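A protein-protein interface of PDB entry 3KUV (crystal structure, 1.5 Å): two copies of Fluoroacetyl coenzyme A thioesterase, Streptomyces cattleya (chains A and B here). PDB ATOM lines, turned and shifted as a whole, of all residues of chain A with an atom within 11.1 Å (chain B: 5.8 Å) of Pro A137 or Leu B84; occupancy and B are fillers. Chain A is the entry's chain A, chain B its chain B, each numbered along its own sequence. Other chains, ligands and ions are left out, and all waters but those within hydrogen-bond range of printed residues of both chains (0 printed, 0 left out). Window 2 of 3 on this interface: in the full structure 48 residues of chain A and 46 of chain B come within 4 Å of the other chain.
Of the 13 printed residues of chain B, 7 touch a printed residue of chain A.
Hydrophobic or aromatic side chains of chain B within 4 Å of the printed part of chain A: Phe B15, Pro B81 and Leu B84.
Of the 10 printed residues of chain A, 5 touch a printed residue of chain B.
Printed residues of chain A that touch a printed residue of chain B: Tyr A27, Val A132, Lys A135, Thr A136 and Pro A137.
Among the printed residues, 10 pairs touch across the chains.
Among the printed residues, Asp or Glu carboxylates within 4 Å of a Lys or Arg side-chain nitrogen of the other chain: Lys A135 with Asp B108 (2.7 Å).
Of the printed residues of chain A, Leu B84 touches Lys A135 (3.5 Å) and Pro A137 (3.99 Å).
Val B16 touches none of the printed residues of chain A.
No residue of chain A comes within 4 Å of Val B17.
Of chain A, only Val A132 (3.8 Å), Lys A135 (3.8 Å) and Thr A136 (3.4 Å) come within 4 Å of Pro B81.
Of chain A, only Pro A137 comes within 4 Å of Pro B82.
Gly B83 touches just one residue of chain A: Pro A137.
Thr B85 touches none of the printed residues of chain A.
Of the printed residues of chain B, Val A132 touches Pro B81.
Of the printed residues of chain B, Lys A135 touches Ala B79 (2.8 Å), Pro B81 (3.8 Å), Leu B84 (3.5 Å) and Asp B108 (2.7 Å).
Of the printed residues of chain B, Tyr A27 touches Phe B15.
Of the printed residues of chain A, Ala B79 touches Lys A135.
Printed residues of chain A within 4 Å of Phe B15: Tyr A27 (3.7 Å).
Val B86 touches none of the printed residues of chain A.
Asn A129 touches none of the printed residues of chain B.
The nearest printed residue of chain B that does not touch Pro A137 is Pro B81 (4.7 Å).
O of Ala B79 is in hydrogen-bond range of NZ of Lys A135 (2.8 Å).
NZ of Lys A135 is in salt-bridge range of OD2 of Asp B108, 2.7 Å away.
No position is printed for both chains.
Of the 10 pairs that touch across the chains among the printed residues, none has its exchanged pair printed and touching as well.
The backbone carbonyl oxygen (O) of Val A132 sits at hydrogen-bond distance from the side-chain hydroxyl (OG1) of Thr A136 (2.8 Å).
The backbone NH (N) of Val B86 is in hydrogen-bond range of the backbone carbonyl oxygen (O) of Phe B15, 2.8 Å away.
The backbone carbonyl oxygen (O) of Val B17 is in hydrogen-bond range of the backbone NH (N) of Gly B83.
O of Leu B84 is in hydrogen-bond range of N of Val B17 (2.9 Å).
OD2 of Asp B108 lies within hydrogen-bond range of OG1 of Thr B80.
N of Val B110 sits at hydrogen-bond distance from OD1 of Asp B108, 3.0 Å away.
Among the printed residues, merely in contact across the chains: Thr A136 with Pro B81 (3.4 Å), Lys A135 with Leu B84 (3.5 Å), Pro A137 with Gly B83 (3.7 Å), Tyr A27 with Phe B15 (3.7 Å), Lys A135 with Pro B81 (3.8 Å), Val A132 with Pro B81 (3.8 Å), Pro A137 with Pro B82 (3.8 Å) and Pro A137 with Leu B84 (3.99 Å).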
ATOM      1  N   TYR A  27     -12.386 -11.827  30.180  1.00  0.00           N
ATOM      2  CA  TYR A  27     -13.111 -10.549  29.908  1.00  0.00           C
ATOM      3  C   TYR A  27     -13.960 -10.126  31.135  1.00  0.00           C
ATOM      4  O   TYR A  27     -15.187 -10.445  31.204  1.00  0.00           O
ATOM      5  CB  TYR A  27     -14.051 -10.667  28.675  1.00  0.00           C
ATOM      6  CG  TYR A  27     -13.266 -10.450  27.393  1.00  0.00           C
ATOM      7  CD1 TYR A  27     -12.999  -9.183  26.945  1.00  0.00           C
ATOM      8  CD2 TYR A  27     -12.742 -11.578  26.682  1.00  0.00           C
ATOM      9  CE1 TYR A  27     -12.294  -8.971  25.735  1.00  0.00           C
ATOM     10  CE2 TYR A  27     -11.994 -11.392  25.494  1.00  0.00           C
ATOM     11  CZ  TYR A  27     -11.789 -10.123  25.036  1.00  0.00           C
ATOM     12  OH  TYR A  27     -11.030  -9.921  23.910  1.00  0.00           O
ATOM     13  N   ASN A 129       6.960  -2.902  14.821  1.00  0.00           N
ATOM     14  CA  ASN A 129       6.480  -1.816  15.705  1.00  0.00           C
ATOM     15  C   ASN A 129       6.210  -0.503  14.952  1.00  0.00           C
ATOM     16  O   ASN A 129       5.192   0.187  15.247  1.00  0.00           O
ATOM     17  CB  ASN A 129       7.415  -1.617  16.857  1.00  0.00           C
ATOM     18  CG  ASN A 129       7.444  -2.775  17.752  1.00  0.00           C
ATOM     19  OD1 ASN A 129       6.443  -3.470  17.969  1.00  0.00           O
ATOM     20  ND2 ASN A 129       8.633  -3.042  18.311  1.00  0.00           N
ATOM     21  N   ALA A 130       7.020  -0.140  13.936  1.00  0.00           N
ATOM     22  CA  ALA A 130       6.694   1.053  13.156  1.00  0.00           C
ATOM     23  C   ALA A 130       5.367   0.958  12.395  1.00  0.00           C
ATOM     24  O   ALA A 130       4.655   1.960  12.248  1.00  0.00           O
ATOM     25  CB  ALA A 130       7.858   1.386  12.152  1.00  0.00           C
ATOM     26  N   LYS A 131       5.057  -0.226  11.878  1.00  0.00           N
ATOM     27  CA  LYS A 131       3.831  -0.389  11.100  1.00  0.00           C
ATOM     28  C   LYS A 131       2.677  -0.269  12.095  1.00  0.00           C
ATOM     29  O   LYS A 131       1.608   0.242  11.729  1.00  0.00           O
ATOM     30  CB  LYS A 131       3.815  -1.754  10.424  1.00  0.00           C
ATOM     31  CG  LYS A 131       4.871  -1.916   9.314  1.00  0.00           C
ATOM     32  CD  LYS A 131       4.342  -2.867   8.261  1.00  0.00           C
ATOM     33  CE  LYS A 131       5.143  -2.747   6.971  1.00  0.00           C
ATOM     34  NZ  LYS A 131       4.721  -1.554   6.119  1.00  0.00           N
ATOM     35  N   VAL A 132       2.900  -0.782  13.304  1.00  0.00           N
ATOM     36  CA  VAL A 132       1.833  -0.767  14.357  1.00  0.00           C
ATOM     37  C   VAL A 132       1.567   0.694  14.711  1.00  0.00           C
ATOM     38  O   VAL A 132       0.415   1.109  14.781  1.00  0.00           O
ATOM     39  CB  VAL A 132       2.168  -1.583  15.596  1.00  0.00           C
ATOM     40  CG1 VAL A 132       1.108  -1.346  16.753  1.00  0.00           C
ATOM     41  CG2 VAL A 132       2.245  -3.103  15.279  1.00  0.00           C
ATOM     42  N   ARG A 133       2.658   1.458  14.930  1.00  0.00           N
ATOM     43  CA  ARG A 133       2.507   2.913  15.261  1.00  0.00           C
ATOM     44  C   ARG A 133       1.725   3.663  14.232  1.00  0.00           C
ATOM     45  O   ARG A 133       0.966   4.593  14.597  1.00  0.00           O
ATOM     46  CB  ARG A 133       3.872   3.586  15.496  1.00  0.00           C
ATOM     47  CG  ARG A 133       4.560   3.034  16.718  1.00  0.00           C
ATOM     48  CD  ARG A 133       5.669   3.951  17.251  1.00  0.00           C
ATOM     49  NE  ARG A 133       6.643   3.089  17.901  1.00  0.00           N
ATOM     50  CZ  ARG A 133       7.718   2.603  17.280  1.00  0.00           C
ATOM     51  NH1 ARG A 133       8.535   1.763  17.915  1.00  0.00           N
ATOM     52  NH2 ARG A 133       7.967   2.981  16.033  1.00  0.00           N
ATOM     53  N   GLN A 134       1.849   3.318  12.955  1.00  0.00           N
ATOM     54  CA  GLN A 134       1.099   4.107  11.992  1.00  0.00           C
ATOM     55  C   GLN A 134      -0.391   3.870  11.915  1.00  0.00           C
ATOM     56  O   GLN A 134      -1.095   4.648  11.245  1.00  0.00           O
ATOM     57  CB  GLN A 134       1.686   4.136  10.610  1.00  0.00           C
ATOM     58  CG  GLN A 134       1.763   2.907   9.883  1.00  0.00           C
ATOM     59  CD  GLN A 134       2.913   3.032   8.901  1.00  0.00           C
ATOM     60  OE1 GLN A 134       3.629   4.047   8.927  1.00  0.00           O
ATOM     61  NE2 GLN A 134       3.102   2.023   8.039  1.00  0.00           N
ATOM     62  N   LYS A 135      -0.849   2.777  12.563  1.00  0.00           N
ATOM     63  CA  LYS A 135      -2.290   2.569  12.696  1.00  0.00           C
ATOM     64  C   LYS A 135      -2.754   2.754  14.146  1.00  0.00           C
ATOM     65  O   LYS A 135      -3.890   2.441  14.437  1.00  0.00           O
ATOM     66  CB  LYS A 135      -2.778   1.220  12.106  1.00  0.00           C
ATOM     67  CG  LYS A 135      -2.084   0.036  12.703  1.00  0.00           C
ATOM     68  CD  LYS A 135      -2.537  -1.362  12.096  1.00  0.00           C
ATOM     69  CE  LYS A 135      -4.009  -1.669  12.367  1.00  0.00           C
ATOM     70  NZ  LYS A 135      -4.308  -3.098  11.899  1.00  0.00           N
ATOM     71  N   THR A 136      -1.927   3.355  15.018  1.00  0.00           N
ATOM     72  CA  THR A 136      -2.276   3.633  16.391  1.00  0.00           C
ATOM     73  C   THR A 136      -2.905   5.056  16.470  1.00  0.00           C
ATOM     74  O   THR A 136      -2.275   6.017  15.974  1.00  0.00           O
ATOM     75  CB  THR A 136      -1.061   3.595  17.299  1.00  0.00           C
ATOM     76  OG1 THR A 136      -0.412   2.295  17.168  1.00  0.00           O
ATOM     77  CG2 THR A 136      -1.441   3.837  18.734  1.00  0.00           C
ATOM     78  N   PRO A 137      -4.142   5.179  17.050  1.00  0.00           N
ATOM     79  CA  PRO A 137      -4.750   6.549  17.169  1.00  0.00           C
ATOM     80  C   PRO A 137      -3.891   7.487  18.022  1.00  0.00           C
ATOM     81  O   PRO A 137      -3.274   7.058  18.983  1.00  0.00           O
ATOM     82  CB  PRO A 137      -6.117   6.312  17.862  1.00  0.00           C
ATOM     83  CG  PRO A 137      -6.357   4.820  17.802  1.00  0.00           C
ATOM     84  CD  PRO A 137      -4.967   4.138  17.720  1.00  0.00           C
ATOM     85  N   PHE B  15     -15.860  -3.505  19.946  1.00  0.00           N
ATOM     86  CA  PHE B  15     -15.075  -3.484  21.180  1.00  0.00           C
ATOM     87  C   PHE B  15     -13.865  -2.631  20.979  1.00  0.00           C
ATOM     88  O   PHE B  15     -12.979  -2.955  20.162  1.00  0.00           O
ATOM     89  CB  PHE B  15     -14.585  -4.928  21.496  1.00  0.00           C
ATOM     90  CG  PHE B  15     -13.795  -5.002  22.779  1.00  0.00           C
ATOM     91  CD1 PHE B  15     -14.400  -4.774  24.041  1.00  0.00           C
ATOM     92  CD2 PHE B  15     -12.440  -5.336  22.704  1.00  0.00           C
ATOM     93  CE1 PHE B  15     -13.548  -4.912  25.241  1.00  0.00           C
ATOM     94  CE2 PHE B  15     -11.691  -5.494  23.855  1.00  0.00           C
ATOM     95  CZ  PHE B  15     -12.225  -5.278  25.090  1.00  0.00           C
ATOM     96  N   VAL B  16     -13.784  -1.499  21.693  1.00  0.00           N
ATOM     97  CA  VAL B  16     -12.553  -0.684  21.649  1.00  0.00           C
ATOM     98  C   VAL B  16     -11.459  -1.401  22.454  1.00  0.00           C
ATOM     99  O   VAL B  16     -11.659  -1.706  23.633  1.00  0.00           O
ATOM    100  CB  VAL B  16     -12.837   0.702  22.272  1.00  0.00           C
ATOM    101  CG1 VAL B  16     -11.515   1.604  22.303  1.00  0.00           C
ATOM    102  CG2 VAL B  16     -13.886   1.440  21.424  1.00  0.00           C
ATOM    103  N   VAL B  17     -10.315  -1.735  21.796  1.00  0.00           N
ATOM    104  CA  VAL B  17      -9.287  -2.479  22.518  1.00  0.00           C
ATOM    105  C   VAL B  17      -8.585  -1.578  23.566  1.00  0.00           C
ATOM    106  O   VAL B  17      -7.983  -0.576  23.163  1.00  0.00           O
ATOM    107  CB  VAL B  17      -8.213  -2.981  21.474  1.00  0.00           C
ATOM    108  CG1 VAL B  17      -7.039  -3.761  22.178  1.00  0.00           C
ATOM    109  CG2 VAL B  17      -8.876  -3.922  20.392  1.00  0.00           C
ATOM    110  N   ALA B  79      -2.291  -6.998  12.875  1.00  0.00           N
ATOM    111  CA  ALA B  79      -2.183  -6.776  14.282  1.00  0.00           C
ATOM    112  C   ALA B  79      -2.839  -5.418  14.652  1.00  0.00           C
ATOM    113  O   ALA B  79      -2.927  -4.488  13.832  1.00  0.00           O
ATOM    114  CB  ALA B  79      -0.712  -6.783  14.716  1.00  0.00           C
ATOM    115  N   THR B  80      -3.347  -5.368  15.899  1.00  0.00           N
ATOM    116  CA  THR B  80      -4.199  -4.213  16.308  1.00  0.00           C
ATOM    117  C   THR B  80      -3.677  -3.643  17.626  1.00  0.00           C
ATOM    118  O   THR B  80      -3.649  -4.302  18.641  1.00  0.00           O
ATOM    119  CB  THR B  80      -5.659  -4.722  16.569  1.00  0.00           C
ATOM    120  OG1 THR B  80      -6.193  -5.319  15.365  1.00  0.00           O
ATOM    121  CG2 THR B  80      -6.642  -3.611  17.018  1.00  0.00           C
ATOM    122  N   PRO B  81      -3.259  -2.361  17.630  1.00  0.00           N
ATOM    123  CA  PRO B  81      -2.878  -1.688  18.891  1.00  0.00           C
ATOM    124  C   PRO B  81      -4.092  -1.285  19.692  1.00  0.00           C
ATOM    125  O   PRO B  81      -5.188  -1.112  19.123  1.00  0.00           O
ATOM    126  CB  PRO B  81      -2.216  -0.392  18.348  1.00  0.00           C
ATOM    127  CG  PRO B  81      -2.932  -0.094  17.053  1.00  0.00           C
ATOM    128  CD  PRO B  81      -3.257  -1.495  16.442  1.00  0.00           C
ATOM    129  N   PRO B  82      -3.884  -1.037  20.959  1.00  0.00           N
ATOM    130  CA  PRO B  82      -5.000  -0.471  21.798  1.00  0.00           C
ATOM    131  C   PRO B  82      -5.481   0.844  21.213  1.00  0.00           C
ATOM    132  O   PRO B  82      -4.756   1.616  20.580  1.00  0.00           O
ATOM    133  CB  PRO B  82      -4.342  -0.230  23.140  1.00  0.00           C
ATOM    134  CG  PRO B  82      -3.157  -1.270  23.173  1.00  0.00           C
ATOM    135  CD  PRO B  82      -2.660  -1.279  21.770  1.00  0.00           C
ATOM    136  N   GLY B  83      -6.770   1.022  21.311  1.00  0.00           N
ATOM    137  CA  GLY B  83      -7.425   2.277  20.924  1.00  0.00           C
ATOM    138  C   GLY B  83      -8.227   2.168  19.641  1.00  0.00           C
ATOM    139  O   GLY B  83      -9.189   2.988  19.395  1.00  0.00           O
ATOM    140  N   LEU B  84      -7.962   1.163  18.800  1.00  0.00           N
ATOM    141  CA  LEU B  84      -8.857   0.868  17.652  1.00  0.00           C
ATOM    142  C   LEU B  84     -10.077   0.073  18.118  1.00  0.00           C
ATOM    143  O   LEU B  84     -10.033  -0.544  19.165  1.00  0.00           O
ATOM    144  CB  LEU B  84      -8.117   0.021  16.540  1.00  0.00           C
ATOM    145  CG  LEU B  84      -7.021   0.860  15.860  1.00  0.00           C
ATOM    146  CD1 LEU B  84      -6.380  -0.036  14.841  1.00  0.00           C
ATOM    147  CD2 LEU B  84      -7.526   2.104  15.123  1.00  0.00           C
ATOM    148  N   THR B  85     -11.147   0.128  17.311  1.00  0.00           N
ATOM    149  CA  THR B  85     -12.350  -0.654  17.618  1.00  0.00           C
ATOM    150  C   THR B  85     -12.264  -1.945  16.763  1.00  0.00           C
ATOM    151  O   THR B  85     -12.199  -1.857  15.514  1.00  0.00           O
ATOM    152  CB  THR B  85     -13.589   0.103  17.206  1.00  0.00           C
ATOM    153  OG1 THR B  85     -13.641   1.380  17.917  1.00  0.00           O
ATOM    154  CG2 THR B  85     -14.880  -0.658  17.504  1.00  0.00           C
ATOM    155  N   VAL B  86     -12.326  -3.072  17.432  1.00  0.00           N
ATOM    156  CA  VAL B  86     -12.424  -4.362  16.732  1.00  0.00           C
ATOM    157  C   VAL B  86     -13.942  -4.639  16.577  1.00  0.00           C
ATOM    158  O   VAL B  86     -14.725  -4.627  17.591  1.00  0.00           O
ATOM    159  CB  VAL B  86     -11.729  -5.485  17.498  1.00  0.00           C
ATOM    160  CG1 VAL B  86     -12.090  -6.868  16.806  1.00  0.00           C
ATOM    161  CG2 VAL B  86     -10.241  -5.251  17.439  1.00  0.00           C
ATOM    162  N   ASP B 108     -10.483  -4.147  12.338  1.00  0.00           N
ATOM    163  CA  ASP B 108     -10.219  -3.129  13.371  1.00  0.00           C
ATOM    164  C   ASP B 108     -10.465  -1.690  12.908  1.00  0.00           C
ATOM    165  O   ASP B 108      -9.896  -0.766  13.486  1.00  0.00           O
ATOM    166  CB  ASP B 108      -8.810  -3.279  13.994  1.00  0.00           C
ATOM    167  CG  ASP B 108      -7.682  -3.120  12.962  1.00  0.00           C
ATOM    168  OD1 ASP B 108      -7.925  -2.617  11.859  1.00  0.00           O
ATOM    169  OD2 ASP B 108      -6.539  -3.495  13.379  1.00  0.00           O
ATOM    170  N   VAL B 110      -9.213  -0.463  10.280  1.00  0.00           N
ATOM    171  CA  VAL B 110      -8.108  -0.197   9.341  1.00  0.00           C
ATOM    172  C   VAL B 110      -7.911  -1.395   8.455  1.00  0.00           C
ATOM    173  O   VAL B 110      -8.005  -1.296   7.198  1.00  0.00           O
ATOM    174  CB  VAL B 110      -6.833   0.131  10.101  1.00  0.00           C
ATOM    175  CG1 VAL B 110      -5.707   0.365   9.073  1.00  0.00           C
ATOM    176  CG2 VAL B 110      -7.083   1.373  10.999  1.00  0.00           C
